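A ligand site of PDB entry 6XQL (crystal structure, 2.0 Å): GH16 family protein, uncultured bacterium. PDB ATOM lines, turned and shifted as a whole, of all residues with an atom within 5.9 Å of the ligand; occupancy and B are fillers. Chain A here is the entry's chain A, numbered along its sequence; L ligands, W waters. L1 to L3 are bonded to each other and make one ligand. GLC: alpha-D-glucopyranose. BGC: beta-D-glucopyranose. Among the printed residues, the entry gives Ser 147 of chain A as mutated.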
ATOM      1  N   TYR A  55      21.094  21.414 -20.145  1.00  0.00           N
ATOM      2  CA  TYR A  55      20.516  20.120 -20.583  1.00  0.00           C
ATOM      3  C   TYR A  55      21.479  19.546 -21.601  1.00  0.00           C
ATOM      4  O   TYR A  55      22.480  20.165 -21.873  1.00  0.00           O
ATOM      5  CB  TYR A  55      19.087  20.309 -21.094  1.00  0.00           C
ATOM      6  CG  TYR A  55      18.191  21.125 -20.194  1.00  0.00           C
ATOM      7  CD1 TYR A  55      17.537  20.548 -19.109  1.00  0.00           C
ATOM      8  CD2 TYR A  55      17.983  22.461 -20.444  1.00  0.00           C
ATOM      9  CE1 TYR A  55      16.681  21.282 -18.306  1.00  0.00           C
ATOM     10  CE2 TYR A  55      17.160  23.224 -19.619  1.00  0.00           C
ATOM     11  CZ  TYR A  55      16.503  22.635 -18.568  1.00  0.00           C
ATOM     12  OH  TYR A  55      15.690  23.411 -17.795  1.00  0.00           O
ATOM     13  N   ASN A  56      21.201  18.338 -22.053  1.00  0.00           N
ATOM     14  CA  ASN A  56      22.006  17.562 -23.026  1.00  0.00           C
ATOM     15  C   ASN A  56      23.400  17.275 -22.426  1.00  0.00           C
ATOM     16  O   ASN A  56      24.349  17.098 -23.201  1.00  0.00           O
ATOM     17  CB  ASN A  56      22.000  18.285 -24.370  1.00  0.00           C
ATOM     18  CG  ASN A  56      20.591  18.657 -24.795  1.00  0.00           C
ATOM     19  OD1 ASN A  56      19.697  17.807 -24.852  1.00  0.00           O
ATOM     20  ND2 ASN A  56      20.376  19.928 -25.056  1.00  0.00           N
ATOM     21  N   GLU A  58      25.294  19.296 -21.376  1.00  0.00           N
ATOM     22  CA  GLU A  58      26.153  20.361 -21.957  1.00  0.00           C
ATOM     23  C   GLU A  58      27.175  20.881 -20.935  1.00  0.00           C
ATOM     24  O   GLU A  58      26.904  20.803 -19.707  1.00  0.00           O
ATOM     25  CB  GLU A  58      25.333  21.516 -22.521  1.00  0.00           C
ATOM     26  CG  GLU A  58      24.626  21.151 -23.818  1.00  0.00           C
ATOM     27  CD  GLU A  58      23.537  22.149 -24.195  1.00  0.00           C
ATOM     28  OE1 GLU A  58      23.545  23.317 -23.630  1.00  0.00           O
ATOM     29  OE2 GLU A  58      22.717  21.803 -25.096  1.00  0.00           O
ATOM     30  N   LYS A 101      24.328  32.530 -24.960  1.00  0.00           N
ATOM     31  CA  LYS A 101      22.962  32.173 -25.387  1.00  0.00           C
ATOM     32  C   LYS A 101      22.087  33.429 -25.269  1.00  0.00           C
ATOM     33  O   LYS A 101      21.831  33.882 -24.134  1.00  0.00           O
ATOM     34  CB  LYS A 101      22.359  31.052 -24.554  1.00  0.00           C
ATOM     35  CG  LYS A 101      20.935  30.721 -24.990  1.00  0.00           C
ATOM     36  CD  LYS A 101      20.408  29.582 -24.229  1.00  0.00           C
ATOM     37  CE  LYS A 101      18.936  29.315 -24.507  1.00  0.00           C
ATOM     38  NZ  LYS A 101      18.477  28.215 -23.641  1.00  0.00           N
ATOM     39  N   TRP A 128      28.840  23.296 -30.630  1.00  0.00           N
ATOM     40  CA  TRP A 128      27.449  22.964 -31.002  1.00  0.00           C
ATOM     41  C   TRP A 128      26.686  24.264 -31.196  1.00  0.00           C
ATOM     42  O   TRP A 128      25.861  24.663 -30.353  1.00  0.00           O
ATOM     43  CB  TRP A 128      26.859  22.010 -29.958  1.00  0.00           C
ATOM     44  CG  TRP A 128      25.476  21.514 -30.228  1.00  0.00           C
ATOM     45  CD1 TRP A 128      24.693  21.663 -31.347  1.00  0.00           C
ATOM     46  CD2 TRP A 128      24.698  20.745 -29.302  1.00  0.00           C
ATOM     47  NE1 TRP A 128      23.469  21.057 -31.159  1.00  0.00           N
ATOM     48  CE2 TRP A 128      23.462  20.455 -29.925  1.00  0.00           C
ATOM     49  CE3 TRP A 128      24.954  20.256 -28.027  1.00  0.00           C
ATOM     50  CZ2 TRP A 128      22.466  19.740 -29.288  1.00  0.00           C
ATOM     51  CZ3 TRP A 128      23.975  19.514 -27.409  1.00  0.00           C
ATOM     52  CH2 TRP A 128      22.741  19.247 -28.028  1.00  0.00           C
ATOM     53  N   PRO A 129      27.007  25.037 -32.257  1.00  0.00           N
ATOM     54  CA  PRO A 129      26.262  26.246 -32.568  1.00  0.00           C
ATOM     55  C   PRO A 129      24.843  25.854 -32.973  1.00  0.00           C
ATOM     56  O   PRO A 129      24.694  24.859 -33.699  1.00  0.00           O
ATOM     57  CB  PRO A 129      27.020  26.890 -33.711  1.00  0.00           C
ATOM     58  CG  PRO A 129      27.656  25.666 -34.373  1.00  0.00           C
ATOM     59  CD  PRO A 129      28.107  24.823 -33.192  1.00  0.00           C
ATOM     60  N   ALA A 130      23.887  26.645 -32.553  1.00  0.00           N
ATOM     61  CA  ALA A 130      22.467  26.411 -32.866  1.00  0.00           C
ATOM     62  C   ALA A 130      21.796  27.767 -33.152  1.00  0.00           C
ATOM     63  O   ALA A 130      22.186  28.793 -32.508  1.00  0.00           O
ATOM     64  CB  ALA A 130      21.833  25.608 -31.749  1.00  0.00           C
ATOM     65  N   TRP A 132      17.758  28.662 -33.417  1.00  0.00           N
ATOM     66  CA  TRP A 132      16.484  27.955 -33.218  1.00  0.00           C
ATOM     67  C   TRP A 132      15.444  28.814 -32.538  1.00  0.00           C
ATOM     68  O   TRP A 132      15.747  29.965 -32.115  1.00  0.00           O
ATOM     69  CB  TRP A 132      16.732  26.622 -32.491  1.00  0.00           C
ATOM     70  CG  TRP A 132      17.366  26.728 -31.151  1.00  0.00           C
ATOM     71  CD1 TRP A 132      18.601  27.262 -30.908  1.00  0.00           C
ATOM     72  CD2 TRP A 132      16.886  26.219 -29.899  1.00  0.00           C
ATOM     73  NE1 TRP A 132      18.907  27.084 -29.588  1.00  0.00           N
ATOM     74  CE2 TRP A 132      17.873  26.496 -28.932  1.00  0.00           C
ATOM     75  CE3 TRP A 132      15.712  25.611 -29.462  1.00  0.00           C
ATOM     76  CZ2 TRP A 132      17.763  26.144 -27.579  1.00  0.00           C
ATOM     77  CZ3 TRP A 132      15.580  25.262 -28.145  1.00  0.00           C
ATOM     78  CH2 TRP A 132      16.586  25.533 -27.206  1.00  0.00           C
ATOM     79  N   MET A 134      11.749  28.535 -29.979  1.00  0.00           N
ATOM     80  CA  MET A 134      10.770  27.806 -29.141  1.00  0.00           C
ATOM     81  C   MET A 134       9.558  28.687 -29.035  1.00  0.00           C
ATOM     82  O   MET A 134       9.725  29.914 -29.181  1.00  0.00           O
ATOM     83  CB  MET A 134      11.282  27.544 -27.741  1.00  0.00           C
ATOM     84  CG  MET A 134      12.469  26.664 -27.709  1.00  0.00           C
ATOM     85  SD  MET A 134      13.017  26.337 -26.008  1.00  0.00           S
ATOM     86  CE  MET A 134      11.679  25.310 -25.436  1.00  0.00           C
ATOM     87  N   GLY A 141       5.195  22.709 -21.925  1.00  0.00           N
ATOM     88  CA  GLY A 141       6.608  22.278 -21.792  1.00  0.00           C
ATOM     89  C   GLY A 141       7.252  21.857 -23.116  1.00  0.00           C
ATOM     90  O   GLY A 141       6.560  21.651 -24.159  1.00  0.00           O
ATOM     91  N   TRP A 142       8.578  21.722 -23.066  1.00  0.00           N
ATOM     92  CA  TRP A 142       9.393  21.077 -24.115  1.00  0.00           C
ATOM     93  C   TRP A 142       9.303  19.567 -23.903  1.00  0.00           C
ATOM     94  O   TRP A 142       9.392  19.076 -22.784  1.00  0.00           O
ATOM     95  CB  TRP A 142      10.811  21.633 -24.099  1.00  0.00           C
ATOM     96  CG  TRP A 142      11.595  21.266 -25.317  1.00  0.00           C
ATOM     97  CD1 TRP A 142      11.851  22.009 -26.427  1.00  0.00           C
ATOM     98  CD2 TRP A 142      12.213  19.989 -25.534  1.00  0.00           C
ATOM     99  NE1 TRP A 142      12.564  21.294 -27.333  1.00  0.00           N
ATOM    100  CE2 TRP A 142      12.801  20.040 -26.810  1.00  0.00           C
ATOM    101  CE3 TRP A 142      12.296  18.819 -24.779  1.00  0.00           C
ATOM    102  CZ2 TRP A 142      13.506  18.959 -27.339  1.00  0.00           C
ATOM    103  CZ3 TRP A 142      13.002  17.754 -25.297  1.00  0.00           C
ATOM    104  CH2 TRP A 142      13.592  17.820 -26.561  1.00  0.00           C
ATOM    105  N   SER A 147       9.438  23.372 -30.975  1.00  0.00           N
ATOM    106  CA  SER A 147      10.738  24.053 -31.193  1.00  0.00           C
ATOM    107  C   SER A 147      11.271  23.760 -32.587  1.00  0.00           C
ATOM    108  O   SER A 147      10.971  22.703 -33.153  1.00  0.00           O
ATOM    109  CB  SER A 147      11.727  23.738 -30.103  1.00  0.00           C
ATOM    110  OG  SER A 147      12.286  22.481 -30.319  1.00  0.00           O
ATOM    111  N   ASP A 149      14.573  23.968 -34.987  1.00  0.00           N
ATOM    112  CA  ASP A 149      16.044  24.075 -35.151  1.00  0.00           C
ATOM    113  C   ASP A 149      16.286  24.475 -36.589  1.00  0.00           C
ATOM    114  O   ASP A 149      16.281  23.565 -37.436  1.00  0.00           O
ATOM    115  CB  ASP A 149      16.702  22.767 -34.793  1.00  0.00           C
ATOM    116  CG  ASP A 149      16.530  22.465 -33.329  1.00  0.00           C
ATOM    117  OD1 ASP A 149      17.054  23.245 -32.527  1.00  0.00           O
ATOM    118  OD2 ASP A 149      15.906  21.452 -33.026  1.00  0.00           O
ATOM    119  N   GLU A 152      21.419  23.594 -36.656  1.00  0.00           N
ATOM    120  CA  GLU A 152      22.349  23.017 -35.675  1.00  0.00           C
ATOM    121  C   GLU A 152      23.535  22.481 -36.460  1.00  0.00           C
ATOM    122  O   GLU A 152      23.319  21.880 -37.519  1.00  0.00           O
ATOM    123  CB  GLU A 152      21.685  21.909 -34.883  1.00  0.00           C
ATOM    124  CG  GLU A 152      20.754  22.370 -33.786  1.00  0.00           C
ATOM    125  CD  GLU A 152      20.092  21.140 -33.185  1.00  0.00           C
ATOM    126  OE1 GLU A 152      19.187  20.622 -33.805  1.00  0.00           O
ATOM    127  OE2 GLU A 152      20.532  20.661 -32.121  1.00  0.00           O
ATOM    128  N   HIS A 166      10.847  19.768 -33.310  1.00  0.00           N
ATOM    129  CA  HIS A 166      10.486  18.945 -32.125  1.00  0.00           C
ATOM    130  C   HIS A 166       9.084  19.356 -31.676  1.00  0.00           C
ATOM    131  O   HIS A 166       8.844  20.534 -31.571  1.00  0.00           O
ATOM    132  CB  HIS A 166      11.529  19.116 -31.024  1.00  0.00           C
ATOM    133  CG  HIS A 166      12.935  18.861 -31.482  1.00  0.00           C
ATOM    134  ND1 HIS A 166      13.540  17.630 -31.354  1.00  0.00           N
ATOM    135  CD2 HIS A 166      13.832  19.683 -32.043  1.00  0.00           C
ATOM    136  CE1 HIS A 166      14.754  17.702 -31.850  1.00  0.00           C
ATOM    137  NE2 HIS A 166      14.986  18.973 -32.235  1.00  0.00           N
ATOM    138  N   HIS A 172      13.573  14.391 -30.114  1.00  0.00           N
ATOM    139  CA  HIS A 172      14.831  13.603 -30.013  1.00  0.00           C
ATOM    140  C   HIS A 172      14.744  12.688 -28.801  1.00  0.00           C
ATOM    141  O   HIS A 172      15.381  11.646 -28.831  1.00  0.00           O
ATOM    142  CB  HIS A 172      16.098  14.481 -29.987  1.00  0.00           C
ATOM    143  CG  HIS A 172      16.367  15.238 -28.724  1.00  0.00           C
ATOM    144  ND1 HIS A 172      16.899  14.644 -27.605  1.00  0.00           N
ATOM    145  CD2 HIS A 172      16.247  16.543 -28.422  1.00  0.00           C
ATOM    146  CE1 HIS A 172      17.038  15.539 -26.641  1.00  0.00           C
ATOM    147  NE2 HIS A 172      16.657  16.733 -27.126  1.00  0.00           N
ATOM    148  N   VAL A 173      14.006  13.087 -27.769  1.00  0.00           N
ATOM    149  CA  VAL A 173      13.950  12.364 -26.465  1.00  0.00           C
ATOM    150  C   VAL A 173      13.459  10.941 -26.709  1.00  0.00           C
ATOM    151  O   VAL A 173      13.954  10.031 -26.036  1.00  0.00           O
ATOM    152  CB  VAL A 173      13.051  13.089 -25.458  1.00  0.00           C
ATOM    153  CG1 VAL A 173      12.907  12.285 -24.166  1.00  0.00           C
ATOM    154  CG2 VAL A 173      13.503  14.517 -25.198  1.00  0.00           C
ATOM    155  N   ASN A 237      22.944  30.433 -29.782  1.00  0.00           N
ATOM    156  CA  ASN A 237      23.868  29.889 -28.777  1.00  0.00           C
ATOM    157  C   ASN A 237      24.974  29.083 -29.440  1.00  0.00           C
ATOM    158  O   ASN A 237      24.853  28.569 -30.581  1.00  0.00           O
ATOM    159  CB  ASN A 237      23.125  29.023 -27.760  1.00  0.00           C
ATOM    160  CG  ASN A 237      22.524  27.775 -28.375  1.00  0.00           C
ATOM    161  OD1 ASN A 237      21.432  27.832 -28.949  1.00  0.00           O
ATOM    162  ND2 ASN A 237      23.153  26.637 -28.141  1.00  0.00           N
ATOM    163  N   ALA A 239      26.571  25.830 -27.742  1.00  0.00           N
ATOM    164  CA  ALA A 239      26.626  24.783 -26.711  1.00  0.00           C
ATOM    165  C   ALA A 239      27.974  24.104 -26.875  1.00  0.00           C
ATOM    166  O   ALA A 239      28.627  24.235 -27.966  1.00  0.00           O
ATOM    167  CB  ALA A 239      25.456  23.802 -26.835  1.00  0.00           C
HETATM  168  C1  GLC L   1      17.885  20.663 -30.144  1.00  0.00           C
HETATM  169  C2  GLC L   1      18.382  20.245 -28.784  1.00  0.00           C
HETATM  170  C3  GLC L   1      17.908  21.209 -27.713  1.00  0.00           C
HETATM  171  C4  GLC L   1      18.943  22.220 -28.031  1.00  0.00           C
HETATM  172  C5  GLC L   1      18.450  22.876 -29.339  1.00  0.00           C
HETATM  173  C6  GLC L   1      19.611  23.636 -29.962  1.00  0.00           C
HETATM  174  O1  GLC L   1      16.497  20.951 -30.071  1.00  0.00           O
HETATM  175  O2  GLC L   1      18.019  19.004 -28.469  1.00  0.00           O
HETATM  176  O3  GLC L   1      17.823  20.614 -26.426  1.00  0.00           O
HETATM  177  O4  GLC L   1      19.155  23.089 -26.960  1.00  0.00           O
HETATM  178  O5  GLC L   1      18.449  21.883 -30.396  1.00  0.00           O
HETATM  179  O6  GLC L   1      20.722  22.719 -29.986  1.00  0.00           O
HETATM  180  C2  BGC L   2      16.947  19.606 -24.336  1.00  0.00           C
HETATM  181  C3  BGC L   2      15.722  19.577 -23.473  1.00  0.00           C
HETATM  182  C4  BGC L   2      15.313  21.016 -23.156  1.00  0.00           C
HETATM  183  C5  BGC L   2      15.117  21.823 -24.431  1.00  0.00           C
HETATM  184  C6  BGC L   2      14.769  23.260 -24.101  1.00  0.00           C
HETATM  185  C1  BGC L   2      16.778  20.474 -25.578  1.00  0.00           C
HETATM  186  O2  BGC L   2      17.234  18.311 -24.762  1.00  0.00           O
HETATM  187  O3  BGC L   2      16.020  18.826 -22.291  1.00  0.00           O
HETATM  188  O4  BGC L   2      14.065  21.120 -22.419  1.00  0.00           O
HETATM  189  O5  BGC L   2      16.339  21.792 -25.227  1.00  0.00           O
HETATM  190  O6  BGC L   2      15.911  23.809 -23.426  1.00  0.00           O
HETATM  191  C2  BGC L   3      12.848  21.642 -20.564  1.00  0.00           C
HETATM  192  C3  BGC L   3      12.670  21.282 -19.106  1.00  0.00           C
HETATM  193  C4  BGC L   3      12.505  19.777 -19.041  1.00  0.00           C
HETATM  194  C5  BGC L   3      13.717  19.113 -19.658  1.00  0.00           C
HETATM  195  C6  BGC L   3      13.606  17.599 -19.723  1.00  0.00           C
HETATM  196  C1  BGC L   3      14.112  20.954 -21.073  1.00  0.00           C
HETATM  197  O2  BGC L   3      13.069  23.036 -20.759  1.00  0.00           O
HETATM  198  O3  BGC L   3      11.534  21.983 -18.721  1.00  0.00           O
HETATM  199  O4  BGC L   3      12.304  19.322 -17.704  1.00  0.00           O
HETATM  200  O5  BGC L   3      13.827  19.578 -21.028  1.00  0.00           O
HETATM  201  O6  BGC L   3      14.877  17.071 -20.163  1.00  0.00           O
HETATM  202  O   HOH W   1      18.499  23.503 -24.360  1.00  0.00           O
HETATM  203  O   HOH W   2      22.131  23.312 -26.933  1.00  0.00           O
HETATM  204  O   HOH W   3      23.232  23.784 -29.450  1.00  0.00           O
HETATM  205  O   HOH W   4      14.829  25.817 -22.111  1.00  0.00           O
HETATM  206  O   HOH W   5      11.367  24.438 -22.086  1.00  0.00           O
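The side-chain amide nitrogen of Asn 56 is in hydrogen-bond range of the side-chain carboxylate of Glu 58.
The indole nitrogen of Trp 142 lies within hydrogen-bond range of the side-chain hydroxyl of Ser 147.
NE2 of His 166 sits at hydrogen-bond distance from OD2 of Asp 149, 2.8 Å away.
The backbone NH (N) of Trp 128 lies within hydrogen-bond range of the backbone carbonyl oxygen (O) of Ala 239 (2.8 Å).
The backbone NH of His 172 is in hydrogen-bond range of a ring nitrogen (ND1) of His 166 (3.5 Å).
N of His 166 lies within hydrogen-bond range of O of Ser 147 (2.9 Å).
The backbone NH of Ala 130 sits at hydrogen-bond distance from the backbone carbonyl oxygen of Asn 237.
NE1 of Trp 132 sits at hydrogen-bond distance from OD1 of Asn 237.
Water W3 lies within hydrogen-bond range of O6 of GLC L1, O of Trp 128 and ND2 of Asn 237.
Water W2 lies within hydrogen-bond range of OE2 of Glu 58 and O4 of GLC L1.
NE2 of His 172 sits at hydrogen-bond distance from O2 of BGC L2, at 2.9 Å.
The side-chain carboxylate (OE2) of Glu 152 lies within hydrogen-bond range of an oxygen (O6) of GLC L1 (3.0 Å).
OD1 of Asn 56 sits at hydrogen-bond distance from O2 of BGC L2 (2.5 Å).
The side-chain carboxylate of Asp 149 sits at hydrogen-bond distance from an oxygen (O1) of GLC L1, at 3.1 Å.
An oxygen (O6) of GLC L1 sits at hydrogen-bond distance from the indole nitrogen (NE1) of Trp 128 (3.4 Å).
NE2 of His 166 sits at hydrogen-bond distance from O1 of GLC L1, 3.3 Å away.
Merely in contact with the ligand: Tyr 55 (3.6 Å), Ala 130 (3.5 Å), Trp 132 (3.4 Å), Met 134 (3.9 Å) and Trp 142 (3.6 Å).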
